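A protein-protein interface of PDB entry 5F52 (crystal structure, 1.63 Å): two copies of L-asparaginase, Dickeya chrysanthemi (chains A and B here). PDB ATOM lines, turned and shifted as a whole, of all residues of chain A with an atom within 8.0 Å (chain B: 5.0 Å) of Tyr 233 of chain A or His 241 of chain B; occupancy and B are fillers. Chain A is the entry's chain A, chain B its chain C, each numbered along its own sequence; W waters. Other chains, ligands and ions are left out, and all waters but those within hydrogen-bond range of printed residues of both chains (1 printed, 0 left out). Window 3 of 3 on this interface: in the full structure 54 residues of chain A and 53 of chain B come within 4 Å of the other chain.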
ATOM      1  N   LEU A 224     -19.376  15.759   0.005  1.00  0.00           N
ATOM      2  CA  LEU A 224     -18.388  16.252  -0.927  1.00  0.00           C
ATOM      3  C   LEU A 224     -18.853  17.595  -1.449  1.00  0.00           C
ATOM      4  O   LEU A 224     -20.053  17.781  -1.738  1.00  0.00           O
ATOM      5  CB  LEU A 224     -18.246  15.284  -2.130  1.00  0.00           C
ATOM      6  CG  LEU A 224     -17.698  13.893  -1.753  1.00  0.00           C
ATOM      7  CD1 LEU A 224     -17.578  13.095  -3.017  1.00  0.00           C
ATOM      8  CD2 LEU A 224     -16.359  13.981  -1.027  1.00  0.00           C
ATOM      9  N   TYR A 227     -17.553  22.801  -6.442  1.00  0.00           N
ATOM     10  CA  TYR A 227     -16.813  24.033  -6.722  1.00  0.00           C
ATOM     11  C   TYR A 227     -16.106  23.890  -8.071  1.00  0.00           C
ATOM     12  O   TYR A 227     -16.081  22.810  -8.645  1.00  0.00           O
ATOM     13  CB  TYR A 227     -15.804  24.313  -5.634  1.00  0.00           C
ATOM     14  CG  TYR A 227     -14.821  23.150  -5.333  1.00  0.00           C
ATOM     15  CD1 TYR A 227     -15.183  22.083  -4.584  1.00  0.00           C
ATOM     16  CD2 TYR A 227     -13.514  23.175  -5.838  1.00  0.00           C
ATOM     17  CE1 TYR A 227     -14.270  21.078  -4.262  1.00  0.00           C
ATOM     18  CE2 TYR A 227     -12.618  22.144  -5.549  1.00  0.00           C
ATOM     19  CZ  TYR A 227     -13.028  21.118  -4.763  1.00  0.00           C
ATOM     20  OH  TYR A 227     -12.167  20.096  -4.387  1.00  0.00           O
ATOM     21  N   ASP A 229     -13.575  23.210 -10.751  1.00  0.00           N
ATOM     22  CA  ASP A 229     -12.465  22.196 -10.781  1.00  0.00           C
ATOM     23  C   ASP A 229     -12.604  21.087  -9.758  1.00  0.00           C
ATOM     24  O   ASP A 229     -11.628  20.391  -9.433  1.00  0.00           O
ATOM     25  CB  ASP A 229     -11.074  22.825 -10.633  1.00  0.00           C
ATOM     26  CG  ASP A 229     -10.786  23.877 -11.676  1.00  0.00           C
ATOM     27  OD1 ASP A 229     -10.746  23.495 -12.855  1.00  0.00           O
ATOM     28  OD2 ASP A 229     -10.653  25.055 -11.328  1.00  0.00           O
ATOM     29  N   ASP A 230     -13.810  20.869  -9.242  1.00  0.00           N
ATOM     30  CA  ASP A 230     -13.996  19.803  -8.255  1.00  0.00           C
ATOM     31  C   ASP A 230     -13.560  18.432  -8.819  1.00  0.00           C
ATOM     32  O   ASP A 230     -13.860  18.137  -9.958  1.00  0.00           O
ATOM     33  CB  ASP A 230     -15.434  19.759  -7.738  1.00  0.00           C
ATOM     34  CG  ASP A 230     -16.473  19.493  -8.808  1.00  0.00           C
ATOM     35  OD1 ASP A 230     -16.280  19.709 -10.020  1.00  0.00           O
ATOM     36  OD2 ASP A 230     -17.565  19.117  -8.370  1.00  0.00           O
ATOM     37  N   PRO A 231     -12.861  17.622  -8.005  1.00  0.00           N
ATOM     38  CA  PRO A 231     -12.220  16.470  -8.588  1.00  0.00           C
ATOM     39  C   PRO A 231     -13.008  15.146  -8.439  1.00  0.00           C
ATOM     40  O   PRO A 231     -13.703  14.903  -7.443  1.00  0.00           O
ATOM     41  CB  PRO A 231     -10.961  16.334  -7.795  1.00  0.00           C
ATOM     42  CG  PRO A 231     -11.383  16.765  -6.406  1.00  0.00           C
ATOM     43  CD  PRO A 231     -12.304  17.942  -6.671  1.00  0.00           C
ATOM     44  N   GLU A 232     -12.938  14.350  -9.490  1.00  0.00           N
ATOM     45  CA  GLU A 232     -13.592  13.063  -9.511  1.00  0.00           C
ATOM     46  C   GLU A 232     -12.965  12.125  -8.479  1.00  0.00           C
ATOM     47  O   GLU A 232     -13.667  11.234  -7.972  1.00  0.00           O
ATOM     48  CB  GLU A 232     -13.473  12.524 -10.949  1.00  0.00           C
ATOM     49  CG  GLU A 232     -14.379  11.391 -11.222  1.00  0.00           C
ATOM     50  CD  GLU A 232     -14.265  10.911 -12.702  1.00  0.00           C
ATOM     51  OE1 GLU A 232     -13.966  11.722 -13.618  1.00  0.00           O
ATOM     52  OE2 GLU A 232     -14.520   9.702 -12.847  1.00  0.00           O
ATOM     53  N   TYR A 233     -11.686  12.303  -8.176  1.00  0.00           N
ATOM     54  CA  TYR A 233     -11.002  11.332  -7.291  1.00  0.00           C
ATOM     55  C   TYR A 233     -11.621  11.284  -5.883  1.00  0.00           C
ATOM     56  O   TYR A 233     -11.450  10.270  -5.178  1.00  0.00           O
ATOM     57  CB  TYR A 233      -9.473  11.596  -7.184  1.00  0.00           C
ATOM     58  CG  TYR A 233      -9.040  12.850  -6.348  1.00  0.00           C
ATOM     59  CD1 TYR A 233      -9.083  12.821  -4.970  1.00  0.00           C
ATOM     60  CD2 TYR A 233      -8.658  14.029  -6.929  1.00  0.00           C
ATOM     61  CE1 TYR A 233      -8.732  13.923  -4.186  1.00  0.00           C
ATOM     62  CE2 TYR A 233      -8.318  15.153  -6.141  1.00  0.00           C
ATOM     63  CZ  TYR A 233      -8.354  15.091  -4.781  1.00  0.00           C
ATOM     64  OH  TYR A 233      -8.030  16.169  -3.972  1.00  0.00           O
ATOM     65  N   LEU A 234     -12.252  12.371  -5.418  1.00  0.00           N
ATOM     66  CA  LEU A 234     -12.878  12.310  -4.118  1.00  0.00           C
ATOM     67  C   LEU A 234     -14.069  11.370  -4.107  1.00  0.00           C
ATOM     68  O   LEU A 234     -14.328  10.679  -3.084  1.00  0.00           O
ATOM     69  CB  LEU A 234     -13.258  13.691  -3.564  1.00  0.00           C
ATOM     70  CG  LEU A 234     -12.057  14.574  -3.274  1.00  0.00           C
ATOM     71  CD1 LEU A 234     -12.527  15.971  -2.951  1.00  0.00           C
ATOM     72  CD2 LEU A 234     -11.221  14.064  -2.117  1.00  0.00           C
ATOM     73  N   TYR A 235     -14.825  11.276  -5.191  1.00  0.00           N
ATOM     74  CA  TYR A 235     -15.885  10.266  -5.335  1.00  0.00           C
ATOM     75  C   TYR A 235     -15.272   8.863  -5.319  1.00  0.00           C
ATOM     76  O   TYR A 235     -15.764   7.983  -4.616  1.00  0.00           O
ATOM     77  CB  TYR A 235     -16.718  10.422  -6.614  1.00  0.00           C
ATOM     78  CG  TYR A 235     -17.526  11.713  -6.618  1.00  0.00           C
ATOM     79  CD1 TYR A 235     -16.927  12.917  -6.957  1.00  0.00           C
ATOM     80  CD2 TYR A 235     -18.821  11.707  -6.211  1.00  0.00           C
ATOM     81  CE1 TYR A 235     -17.654  14.112  -6.918  1.00  0.00           C
ATOM     82  CE2 TYR A 235     -19.551  12.903  -6.147  1.00  0.00           C
ATOM     83  CZ  TYR A 235     -18.941  14.078  -6.532  1.00  0.00           C
ATOM     84  OH  TYR A 235     -19.678  15.228  -6.481  1.00  0.00           O
ATOM     85  N   ASP A 236     -14.229   8.670  -6.087  1.00  0.00           N
ATOM     86  CA  ASP A 236     -13.531   7.351  -6.113  1.00  0.00           C
ATOM     87  C   ASP A 236     -13.084   6.943  -4.715  1.00  0.00           C
ATOM     88  O   ASP A 236     -13.237   5.808  -4.345  1.00  0.00           O
ATOM     89  CB  ASP A 236     -12.290   7.353  -6.991  1.00  0.00           C
ATOM     90  CG  ASP A 236     -12.598   7.623  -8.464  1.00  0.00           C
ATOM     91  OD1 ASP A 236     -13.664   7.259  -8.947  1.00  0.00           O
ATOM     92  OD2 ASP A 236     -11.714   8.223  -9.129  1.00  0.00           O
ATOM     93  N   ALA A 237     -12.532   7.888  -3.961  1.00  0.00           N
ATOM     94  CA  ALA A 237     -12.093   7.610  -2.599  1.00  0.00           C
ATOM     95  C   ALA A 237     -13.287   7.212  -1.659  1.00  0.00           C
ATOM     96  O   ALA A 237     -13.189   6.217  -0.893  1.00  0.00           O
ATOM     97  CB  ALA A 237     -11.325   8.771  -2.036  1.00  0.00           C
ATOM     98  N   ALA A 238     -14.402   7.915  -1.751  1.00  0.00           N
ATOM     99  CA  ALA A 238     -15.517   7.593  -0.939  1.00  0.00           C
ATOM    100  C   ALA A 238     -16.083   6.220  -1.268  1.00  0.00           C
ATOM    101  O   ALA A 238     -16.331   5.398  -0.366  1.00  0.00           O
ATOM    102  CB  ALA A 238     -16.591   8.661  -1.091  1.00  0.00           C
ATOM    103  N   ILE A 239     -16.220   5.931  -2.557  1.00  0.00           N
ATOM    104  CA  ILE A 239     -16.636   4.641  -2.999  1.00  0.00           C
ATOM    105  C   ILE A 239     -15.721   3.507  -2.477  1.00  0.00           C
ATOM    106  O   ILE A 239     -16.188   2.504  -1.915  1.00  0.00           O
ATOM    107  CB  ILE A 239     -16.648   4.548  -4.521  1.00  0.00           C
ATOM    108  CG1 ILE A 239     -17.767   5.443  -5.106  1.00  0.00           C
ATOM    109  CG2 ILE A 239     -16.877   3.112  -4.968  1.00  0.00           C
ATOM    110  CD1 ILE A 239     -17.554   5.695  -6.574  1.00  0.00           C
ATOM    111  N   GLN A 240     -14.447   3.692  -2.631  1.00  0.00           N
ATOM    112  CA  GLN A 240     -13.470   2.710  -2.205  1.00  0.00           C
ATOM    113  C   GLN A 240     -13.580   2.441  -0.696  1.00  0.00           C
ATOM    114  O   GLN A 240     -13.353   1.324  -0.252  1.00  0.00           O
ATOM    115  CB  GLN A 240     -12.069   3.191  -2.540  1.00  0.00           C
ATOM    116  CG  GLN A 240     -10.882   2.294  -2.117  1.00  0.00           C
ATOM    117  CD  GLN A 240     -10.969   0.918  -2.762  1.00  0.00           C
ATOM    118  OE1 GLN A 240     -10.870  -0.105  -2.087  1.00  0.00           O
ATOM    119  NE2 GLN A 240     -11.217   0.890  -4.088  1.00  0.00           N
ATOM    120  N   ARG A 259     -17.180  16.443 -14.079  1.00  0.00           N
ATOM    121  CA  ARG A 259     -16.412  15.568 -13.170  1.00  0.00           C
ATOM    122  C   ARG A 259     -17.294  14.995 -12.082  1.00  0.00           C
ATOM    123  O   ARG A 259     -17.219  13.825 -11.753  1.00  0.00           O
ATOM    124  CB  ARG A 259     -15.230  16.288 -12.608  1.00  0.00           C
ATOM    125  CG  ARG A 259     -14.196  16.730 -13.702  1.00  0.00           C
ATOM    126  CD  ARG A 259     -13.138  17.689 -13.205  1.00  0.00           C
ATOM    127  NE  ARG A 259     -13.786  18.807 -12.549  1.00  0.00           N
ATOM    128  CZ  ARG A 259     -14.386  19.823 -13.158  1.00  0.00           C
ATOM    129  NH1 ARG A 259     -14.283  19.990 -14.472  1.00  0.00           N
ATOM    130  NH2 ARG A 259     -15.038  20.696 -12.452  1.00  0.00           N
ATOM    131  N   GLY A 263     -18.286  11.066 -11.272  1.00  0.00           N
ATOM    132  CA  GLY A 263     -18.177  10.530  -9.931  1.00  0.00           C
ATOM    133  C   GLY A 263     -19.483   9.931  -9.401  1.00  0.00           C
ATOM    134  O   GLY A 263     -19.499   8.876  -8.783  1.00  0.00           O
ATOM    135  N   LYS A 266     -20.437   6.685 -11.156  1.00  0.00           N
ATOM    136  CA  LYS A 266     -19.653   5.611 -10.565  1.00  0.00           C
ATOM    137  C   LYS A 266     -20.175   5.150  -9.234  1.00  0.00           C
ATOM    138  O   LYS A 266     -20.269   3.955  -8.982  1.00  0.00           O
ATOM    139  CB  LYS A 266     -18.199   6.000 -10.430  1.00  0.00           C
ATOM    140  CG  LYS A 266     -17.466   5.841 -11.716  1.00  0.00           C
ATOM    141  CD  LYS A 266     -15.964   5.919 -11.536  1.00  0.00           C
ATOM    142  CE  LYS A 266     -15.513   7.320 -11.693  1.00  0.00           C
ATOM    143  NZ  LYS A 266     -14.036   7.381 -11.629  1.00  0.00           N
ATOM    144  N   LYS B 220      -3.126  23.444  -7.662  1.00  0.00           N
ATOM    145  CA  LYS B 220      -4.325  22.643  -7.402  1.00  0.00           C
ATOM    146  C   LYS B 220      -4.774  22.795  -5.956  1.00  0.00           C
ATOM    147  O   LYS B 220      -3.951  22.582  -5.058  1.00  0.00           O
ATOM    148  CB  LYS B 220      -4.003  21.191  -7.653  1.00  0.00           C
ATOM    149  CG  LYS B 220      -5.188  20.281  -7.514  1.00  0.00           C
ATOM    150  CD  LYS B 220      -4.892  18.883  -8.085  1.00  0.00           C
ATOM    151  CE  LYS B 220      -6.068  17.940  -7.814  1.00  0.00           C
ATOM    152  NZ  LYS B 220      -7.479  18.434  -8.099  1.00  0.00           N
ATOM    153  N   ASP B 222      -8.102  21.859  -3.330  1.00  0.00           N
ATOM    154  CA  ASP B 222      -9.399  21.204  -3.136  1.00  0.00           C
ATOM    155  C   ASP B 222     -10.030  21.691  -1.856  1.00  0.00           C
ATOM    156  O   ASP B 222      -9.410  22.301  -1.035  1.00  0.00           O
ATOM    157  CB  ASP B 222      -9.241  19.691  -3.185  1.00  0.00           C
ATOM    158  CG  ASP B 222      -9.073  19.207  -4.646  1.00  0.00           C
ATOM    159  OD1 ASP B 222      -9.714  19.793  -5.565  1.00  0.00           O
ATOM    160  OD2 ASP B 222      -8.299  18.286  -4.863  1.00  0.00           O
ATOM    161  N   ALA B 237      -6.508  11.204   0.172  1.00  0.00           N
ATOM    162  CA  ALA B 237      -6.787  11.202  -1.267  1.00  0.00           C
ATOM    163  C   ALA B 237      -6.307  12.496  -1.940  1.00  0.00           C
ATOM    164  O   ALA B 237      -5.630  12.485  -2.995  1.00  0.00           O
ATOM    165  CB  ALA B 237      -8.241  10.943  -1.534  1.00  0.00           C
ATOM    166  N   ALA B 238      -6.590  13.626  -1.302  1.00  0.00           N
ATOM    167  CA  ALA B 238      -6.110  14.891  -1.807  1.00  0.00           C
ATOM    168  C   ALA B 238      -4.590  14.935  -1.886  1.00  0.00           C
ATOM    169  O   ALA B 238      -4.018  15.358  -2.893  1.00  0.00           O
ATOM    170  CB  ALA B 238      -6.685  16.041  -0.976  1.00  0.00           C
ATOM    171  N   ILE B 239      -3.914  14.515  -0.828  1.00  0.00           N
ATOM    172  CA  ILE B 239      -2.457  14.494  -0.791  1.00  0.00           C
ATOM    173  C   ILE B 239      -1.921  13.594  -1.912  1.00  0.00           C
ATOM    174  O   ILE B 239      -1.026  14.005  -2.641  1.00  0.00           O
ATOM    175  CB  ILE B 239      -1.962  13.948   0.548  1.00  0.00           C
ATOM    176  CG1 ILE B 239      -2.250  14.941   1.678  1.00  0.00           C
ATOM    177  CG2 ILE B 239      -0.475  13.684   0.517  1.00  0.00           C
ATOM    178  CD1 ILE B 239      -2.193  14.297   3.039  1.00  0.00           C
ATOM    179  N   GLN B 240      -2.479  12.424  -2.057  1.00  0.00           N
ATOM    180  CA  GLN B 240      -2.053  11.461  -3.091  1.00  0.00           C
ATOM    181  C   GLN B 240      -2.241  12.011  -4.500  1.00  0.00           C
ATOM    182  O   GLN B 240      -1.434  11.750  -5.371  1.00  0.00           O
ATOM    183  CB  GLN B 240      -2.852  10.213  -2.938  1.00  0.00           C
ATOM    184  CG  GLN B 240      -2.818   9.233  -4.087  1.00  0.00           C
ATOM    185  CD  GLN B 240      -3.701   8.017  -3.775  1.00  0.00           C
ATOM    186  OE1 GLN B 240      -4.517   8.026  -2.808  1.00  0.00           O
ATOM    187  NE2 GLN B 240      -3.575   6.985  -4.596  1.00  0.00           N
ATOM    188  N   HIS B 241      -3.259  12.822  -4.721  1.00  0.00           N
ATOM    189  CA  HIS B 241      -3.457  13.473  -6.017  1.00  0.00           C
ATOM    190  C   HIS B 241      -2.713  14.777  -6.215  1.00  0.00           C
ATOM    191  O   HIS B 241      -2.970  15.501  -7.160  1.00  0.00           O
ATOM    192  CB  HIS B 241      -4.955  13.579  -6.326  1.00  0.00           C
ATOM    193  CG  HIS B 241      -5.543  12.254  -6.677  1.00  0.00           C
ATOM    194  ND1 HIS B 241      -5.895  11.328  -5.703  1.00  0.00           N
ATOM    195  CD2 HIS B 241      -5.732  11.649  -7.868  1.00  0.00           C
ATOM    196  CE1 HIS B 241      -6.350  10.242  -6.291  1.00  0.00           C
ATOM    197  NE2 HIS B 241      -6.255  10.413  -7.601  1.00  0.00           N
ATOM    198  N   GLY B 242      -1.821  15.123  -5.328  1.00  0.00           N
ATOM    199  CA  GLY B 242      -0.919  16.242  -5.548  1.00  0.00           C
ATOM    200  C   GLY B 242      -1.472  17.615  -5.303  1.00  0.00           C
ATOM    201  O   GLY B 242      -0.985  18.583  -5.863  1.00  0.00           O
ATOM    202  N   VAL B 243      -2.468  17.765  -4.418  1.00  0.00           N
ATOM    203  CA  VAL B 243      -2.925  19.145  -4.133  1.00  0.00           C
ATOM    204  C   VAL B 243      -1.829  19.959  -3.513  1.00  0.00           C
ATOM    205  O   VAL B 243      -0.957  19.435  -2.798  1.00  0.00           O
ATOM    206  CB  VAL B 243      -4.134  19.207  -3.198  1.00  0.00           C
ATOM    207  CG1 VAL B 243      -5.322  18.587  -3.817  1.00  0.00           C
ATOM    208  CG2 VAL B 243      -3.804  18.591  -1.856  1.00  0.00           C
HETATM  209  O   HOH W   1      -9.293  20.809  -7.749  1.00  0.00           O
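Of the printed residues of chain A, His 241 of chain B touches Tyr 233. No residue of chain A comes within 4 Å of Gly 242 of chain B. Of the printed residues of chain A, Asp 222 of chain B touches Tyr 227 (2.7 Å), Pro 231 (3.4 Å) and Tyr 233 (2.3 Å). Of the printed residues of chain B, Tyr 227 of chain A touches Asp 222. Of the printed residues of chain A, Ala 238 of chain B touches Tyr 233. Ile 239 of chain B touches none of the printed residues of chain A.
Among the printed residues, pairs that only touch across the chains: Pro 231 of chain A with Asp 222 of chain B, Tyr 233 of chain A with Lys 220 of chain B, Tyr 233 of chain A with Ala 237 of chain B, Tyr 233 of chain A with Ala 238 of chain B, Tyr 233 of chain A with His 241 of chain B, Tyr 233 of chain A with Val 243 of chain B and Ala 237 of chain A with Ala 237 of chain B.
Water W1 lies within hydrogen-bond range of the side-chain carboxylate of Asp 222 of chain B (2.4 Å), the backbone carbonyl oxygen of Asp 229 of chain A (2.9 Å) and the side-chain amino group of Lys 220 of chain B (3.0 Å).
O of Ala 237 of chain B sits at hydrogen-bond distance from ND1 of His 241 of chain B (3.0 Å). The side-chain carboxylate (OD2) of Asp 222 of chain B is in salt-bridge range of the side-chain amino group (NZ) of Lys 220 of chain B. The backbone carbonyl oxygen of Ala 238 of chain B is in hydrogen-bond range of the backbone NH of Val 243 of chain B (3.2 Å).
OD2 of Asp 222 of chain B sits close to OH of Tyr 233 of chain A, 2.3 Å away. The side-chain hydroxyl (OH) of Tyr 227 of chain A lies within hydrogen-bond range of the side-chain carboxylate (OD1) of Asp 222 of chain B (2.7 Å).
Ala 237 of chain B touches its own counterpart, Ala 237 of chain A. 4 positions are printed for both chains. Of the 9 pairs that touch across the chains among the printed residues, 1 has its exchanged pair printed and touching as well.
Of the 17 printed residues of chain A, 4 touch a printed residue of chain B. Of the 9 printed residues of chain B, 6 touch a printed residue of chain A. Hydrophobic or aromatic side chains of chain B that line the printed part of chain A: Ala 237, Ala 238, His 241 and Val 243. Among the printed residues, no Asp or Glu carboxylate lies within 4 Å of a Lys or Arg side-chain nitrogen of the other chain.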
